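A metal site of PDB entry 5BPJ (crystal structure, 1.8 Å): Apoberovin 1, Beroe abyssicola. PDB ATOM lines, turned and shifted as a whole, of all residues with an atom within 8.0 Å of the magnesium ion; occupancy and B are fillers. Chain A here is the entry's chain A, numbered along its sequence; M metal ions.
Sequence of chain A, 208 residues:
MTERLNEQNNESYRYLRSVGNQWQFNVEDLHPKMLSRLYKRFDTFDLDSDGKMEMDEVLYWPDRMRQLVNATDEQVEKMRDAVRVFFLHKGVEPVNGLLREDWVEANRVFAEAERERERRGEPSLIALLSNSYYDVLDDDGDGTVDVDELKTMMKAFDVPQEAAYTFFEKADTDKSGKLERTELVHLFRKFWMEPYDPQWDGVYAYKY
OD1 of Asp 172 is bound to the magnesium ion, 1.8 Å away. The magnesium ion is bound by OE1 of Glu 180 (2.0 Å). The magnesium ion is bound by OG of Ser 176, at 2.3 Å. O of Lys 178 binds the magnesium ion, at 2.4 Å. OE2 of Glu 183 is bound to the magnesium ion (2.5 Å). OE1 of Glu 183 binds the magnesium ion (2.5 Å). The magnesium ion has six donor atoms within binding distance. Slightly farther from the magnesium ion lies the side-chain carboxylate (OD1) of Asp 174 (2.7 Å).
The side-chain carboxylate (OD2) of Asp 172 is in hydrogen-bond range of the backbone NH (N) of Gly 177. OD1 of Asp 172 sits close to OD1 of Asp 174 (2.7 Å). OD1 of Asp 174 is in hydrogen-bond range of N of Ser 176 (2.8 Å).
Of the 17 residues printed, 6 come within 4 Å of the magnesium ion.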
ATOM      1  N   TYR A 134      -7.984   7.743 -18.805  1.00  0.00           N
ATOM      2  CA  TYR A 134      -8.510   6.925 -19.901  1.00  0.00           C
ATOM      3  C   TYR A 134     -10.031   6.764 -19.828  1.00  0.00           C
ATOM      4  O   TYR A 134     -10.740   6.983 -20.817  1.00  0.00           O
ATOM      5  CB  TYR A 134      -7.806   5.550 -19.919  1.00  0.00           C
ATOM      6  CG  TYR A 134      -8.027   4.745 -21.180  1.00  0.00           C
ATOM      7  CD1 TYR A 134      -9.113   3.887 -21.300  1.00  0.00           C
ATOM      8  CD2 TYR A 134      -7.164   4.846 -22.261  1.00  0.00           C
ATOM      9  CE1 TYR A 134      -9.325   3.132 -22.458  1.00  0.00           C
ATOM     10  CE2 TYR A 134      -7.363   4.095 -23.422  1.00  0.00           C
ATOM     11  CZ  TYR A 134      -8.449   3.249 -23.502  1.00  0.00           C
ATOM     12  OH  TYR A 134      -8.676   2.496 -24.632  1.00  0.00           O
ATOM     13  N   THR A 144     -12.470   3.229 -26.150  1.00  0.00           N
ATOM     14  CA  THR A 144     -11.131   3.654 -26.571  1.00  0.00           C
ATOM     15  C   THR A 144     -11.058   5.176 -26.723  1.00  0.00           C
ATOM     16  O   THR A 144     -12.074   5.849 -26.864  1.00  0.00           O
ATOM     17  CB  THR A 144     -10.735   3.025 -27.900  1.00  0.00           C
ATOM     18  OG1 THR A 144     -11.863   3.045 -28.785  1.00  0.00           O
ATOM     19  CG2 THR A 144     -10.284   1.581 -27.696  1.00  0.00           C
ATOM     20  N   VAL A 145      -9.838   5.696 -26.704  1.00  0.00           N
ATOM     21  CA  VAL A 145      -9.637   7.132 -26.830  1.00  0.00           C
ATOM     22  C   VAL A 145      -9.234   7.495 -28.250  1.00  0.00           C
ATOM     23  O   VAL A 145      -8.328   6.902 -28.821  1.00  0.00           O
ATOM     24  CB  VAL A 145      -8.572   7.636 -25.828  1.00  0.00           C
ATOM     25  CG1 VAL A 145      -8.357   9.150 -25.968  1.00  0.00           C
ATOM     26  CG2 VAL A 145      -8.980   7.248 -24.395  1.00  0.00           C
ATOM     27  N   PHE A 168      -0.514  11.676 -30.242  1.00  0.00           N
ATOM     28  CA  PHE A 168      -1.289  10.546 -30.736  1.00  0.00           C
ATOM     29  C   PHE A 168      -0.505   9.639 -31.674  1.00  0.00           C
ATOM     30  O   PHE A 168      -0.465   8.410 -31.472  1.00  0.00           O
ATOM     31  CB  PHE A 168      -2.571  11.011 -31.413  1.00  0.00           C
ATOM     32  CG  PHE A 168      -3.635   9.964 -31.466  1.00  0.00           C
ATOM     33  CD1 PHE A 168      -3.629   8.998 -32.475  1.00  0.00           C
ATOM     34  CD2 PHE A 168      -4.629   9.918 -30.507  1.00  0.00           C
ATOM     35  CE1 PHE A 168      -4.612   8.027 -32.519  1.00  0.00           C
ATOM     36  CE2 PHE A 168      -5.605   8.958 -30.544  1.00  0.00           C
ATOM     37  CZ  PHE A 168      -5.601   8.001 -31.551  1.00  0.00           C
ATOM     38  N   ALA A 171       1.889   7.527 -29.906  1.00  0.00           N
ATOM     39  CA  ALA A 171       1.350   6.504 -28.997  1.00  0.00           C
ATOM     40  C   ALA A 171       0.577   5.366 -29.681  1.00  0.00           C
ATOM     41  O   ALA A 171       0.385   4.312 -29.072  1.00  0.00           O
ATOM     42  CB  ALA A 171       0.501   7.155 -27.908  1.00  0.00           C
ATOM     43  N   ASP A 172       0.125   5.505 -30.926  1.00  0.00           N
ATOM     44  CA  ASP A 172      -0.643   4.398 -31.562  1.00  0.00           C
ATOM     45  C   ASP A 172       0.183   3.616 -32.507  1.00  0.00           C
ATOM     46  O   ASP A 172       0.204   3.836 -33.668  1.00  0.00           O
ATOM     47  CB  ASP A 172      -1.878   4.877 -32.304  1.00  0.00           C
ATOM     48  CG  ASP A 172      -2.889   3.775 -32.617  1.00  0.00           C
ATOM     49  OD1 ASP A 172      -3.260   2.770 -31.874  1.00  0.00           O
ATOM     50  OD2 ASP A 172      -3.385   4.043 -33.691  1.00  0.00           O
ATOM     51  N   THR A 173       0.919   2.692 -31.924  1.00  0.00           N
ATOM     52  CA  THR A 173       2.021   1.960 -32.545  1.00  0.00           C
ATOM     53  C   THR A 173       1.531   0.790 -33.350  1.00  0.00           C
ATOM     54  O   THR A 173       2.294   0.185 -34.034  1.00  0.00           O
ATOM     55  CB  THR A 173       3.026   1.468 -31.481  1.00  0.00           C
ATOM     56  OG1 THR A 173       2.363   0.795 -30.427  1.00  0.00           O
ATOM     57  CG2 THR A 173       3.745   2.605 -30.884  1.00  0.00           C
ATOM     58  N   ASP A 174       0.255   0.492 -33.207  1.00  0.00           N
ATOM     59  CA  ASP A 174      -0.497  -0.355 -34.136  1.00  0.00           C
ATOM     60  C   ASP A 174      -1.271   0.366 -35.275  1.00  0.00           C
ATOM     61  O   ASP A 174      -1.789  -0.254 -36.137  1.00  0.00           O
ATOM     62  CB  ASP A 174      -1.360  -1.329 -33.391  1.00  0.00           C
ATOM     63  CG  ASP A 174      -2.563  -0.735 -32.798  1.00  0.00           C
ATOM     64  OD1 ASP A 174      -2.844   0.407 -33.049  1.00  0.00           O
ATOM     65  OD2 ASP A 174      -3.238  -1.454 -32.095  1.00  0.00           O
ATOM     66  N   LYS A 175      -1.264   1.684 -35.282  1.00  0.00           N
ATOM     67  CA  LYS A 175      -1.984   2.444 -36.274  1.00  0.00           C
ATOM     68  C   LYS A 175      -3.466   2.173 -36.323  1.00  0.00           C
ATOM     69  O   LYS A 175      -4.081   2.378 -37.315  1.00  0.00           O
ATOM     70  CB  LYS A 175      -1.400   2.251 -37.667  1.00  0.00           C
ATOM     71  CG  LYS A 175      -0.814   3.520 -38.293  1.00  0.00           C
ATOM     72  CD  LYS A 175      -1.453   3.892 -39.619  1.00  0.00           C
ATOM     73  CE  LYS A 175      -0.911   3.126 -40.823  1.00  0.00           C
ATOM     74  NZ  LYS A 175      -1.870   2.156 -41.395  1.00  0.00           N
ATOM     75  N   SER A 176      -4.032   1.759 -35.227  1.00  0.00           N
ATOM     76  CA  SER A 176      -5.451   1.435 -35.133  1.00  0.00           C
ATOM     77  C   SER A 176      -6.334   2.659 -35.375  1.00  0.00           C
ATOM     78  O   SER A 176      -7.411   2.541 -35.938  1.00  0.00           O
ATOM     79  CB  SER A 176      -5.816   0.756 -33.808  1.00  0.00           C
ATOM     80  OG  SER A 176      -5.770   1.636 -32.695  1.00  0.00           O
ATOM     81  N   GLY A 177      -5.858   3.824 -34.966  1.00  0.00           N
ATOM     82  CA  GLY A 177      -6.611   5.061 -35.113  1.00  0.00           C
ATOM     83  C   GLY A 177      -7.193   5.454 -33.771  1.00  0.00           C
ATOM     84  O   GLY A 177      -7.760   6.541 -33.613  1.00  0.00           O
ATOM     85  N   LYS A 178      -7.087   4.552 -32.804  1.00  0.00           N
ATOM     86  CA  LYS A 178      -7.543   4.798 -31.445  1.00  0.00           C
ATOM     87  C   LYS A 178      -6.440   4.417 -30.469  1.00  0.00           C
ATOM     88  O   LYS A 178      -5.695   3.443 -30.697  1.00  0.00           O
ATOM     89  CB  LYS A 178      -8.784   3.957 -31.134  1.00  0.00           C
ATOM     90  CG  LYS A 178      -9.903   4.115 -32.157  1.00  0.00           C
ATOM     91  CD  LYS A 178     -10.455   5.533 -32.152  1.00  0.00           C
ATOM     92  CE  LYS A 178     -11.465   5.736 -33.278  1.00  0.00           C
ATOM     93  NZ  LYS A 178     -10.849   5.742 -34.648  1.00  0.00           N
ATOM     94  N   LEU A 179      -6.312   5.174 -29.389  1.00  0.00           N
ATOM     95  CA  LEU A 179      -5.401   4.774 -28.308  1.00  0.00           C
ATOM     96  C   LEU A 179      -6.116   3.833 -27.358  1.00  0.00           C
ATOM     97  O   LEU A 179      -7.187   4.143 -26.826  1.00  0.00           O
ATOM     98  CB  LEU A 179      -4.884   6.000 -27.541  1.00  0.00           C
ATOM     99  CG  LEU A 179      -3.907   6.904 -28.297  1.00  0.00           C
ATOM    100  CD1 LEU A 179      -3.333   7.978 -27.362  1.00  0.00           C
ATOM    101  CD2 LEU A 179      -2.798   6.075 -28.898  1.00  0.00           C
ATOM    102  N   GLU A 180      -5.454   2.704 -27.117  1.00  0.00           N
ATOM    103  CA  GLU A 180      -5.961   1.756 -26.191  1.00  0.00           C
ATOM    104  C   GLU A 180      -5.175   1.890 -24.904  1.00  0.00           C
ATOM    105  O   GLU A 180      -4.215   2.539 -24.884  1.00  0.00           O
ATOM    106  CB  GLU A 180      -5.951   0.368 -26.820  1.00  0.00           C
ATOM    107  CG  GLU A 180      -6.994   0.248 -27.930  1.00  0.00           C
ATOM    108  CD  GLU A 180      -6.484   0.592 -29.313  1.00  0.00           C
ATOM    109  OE1 GLU A 180      -5.290   0.564 -29.559  1.00  0.00           O
ATOM    110  OE2 GLU A 180      -7.261   0.907 -30.188  1.00  0.00           O
ATOM    111  N   ARG A 181      -5.679   1.319 -23.840  1.00  0.00           N
ATOM    112  CA  ARG A 181      -5.189   1.573 -22.503  1.00  0.00           C
ATOM    113  C   ARG A 181      -3.718   1.542 -22.418  1.00  0.00           C
ATOM    114  O   ARG A 181      -3.125   2.406 -21.872  1.00  0.00           O
ATOM    115  CB  ARG A 181      -5.713   0.582 -21.541  1.00  0.00           C
ATOM    116  CG  ARG A 181      -7.142   0.752 -21.194  1.00  0.00           C
ATOM    117  CD  ARG A 181      -7.338   0.689 -19.731  1.00  0.00           C
ATOM    118  NE  ARG A 181      -8.711   0.595 -19.371  1.00  0.00           N
ATOM    119  CZ  ARG A 181      -9.313   1.406 -18.547  1.00  0.00           C
ATOM    120  NH1 ARG A 181      -8.651   2.360 -17.971  1.00  0.00           N
ATOM    121  NH2 ARG A 181     -10.562   1.226 -18.258  1.00  0.00           N
ATOM    122  N   GLU A 183      -1.429   1.829 -24.704  1.00  0.00           N
ATOM    123  CA  GLU A 183      -0.772   2.885 -25.435  1.00  0.00           C
ATOM    124  C   GLU A 183      -0.794   4.234 -24.696  1.00  0.00           C
ATOM    125  O   GLU A 183       0.154   4.928 -24.702  1.00  0.00           O
ATOM    126  CB  GLU A 183      -1.309   2.985 -26.855  1.00  0.00           C
ATOM    127  CG  GLU A 183      -1.610   1.684 -27.571  1.00  0.00           C
ATOM    128  CD  GLU A 183      -2.365   1.899 -28.855  1.00  0.00           C
ATOM    129  OE1 GLU A 183      -3.441   2.440 -28.742  1.00  0.00           O
ATOM    130  OE2 GLU A 183      -1.905   1.590 -29.939  1.00  0.00           O
ATOM    131  N   LEU A 184      -1.878   4.554 -24.038  1.00  0.00           N
ATOM    132  CA  LEU A 184      -1.937   5.788 -23.238  1.00  0.00           C
ATOM    133  C   LEU A 184      -0.981   5.721 -22.070  1.00  0.00           C
ATOM    134  O   LEU A 184      -0.376   6.702 -21.749  1.00  0.00           O
ATOM    135  CB  LEU A 184      -3.366   6.153 -22.745  1.00  0.00           C
ATOM    136  CG  LEU A 184      -3.607   7.633 -22.439  1.00  0.00           C
ATOM    137  CD1 LEU A 184      -3.297   8.503 -23.600  1.00  0.00           C
ATOM    138  CD2 LEU A 184      -4.986   7.936 -21.905  1.00  0.00           C
HETATM  139 MG    MG M   1      -4.199   1.528 -30.976  1.00  0.00          MG
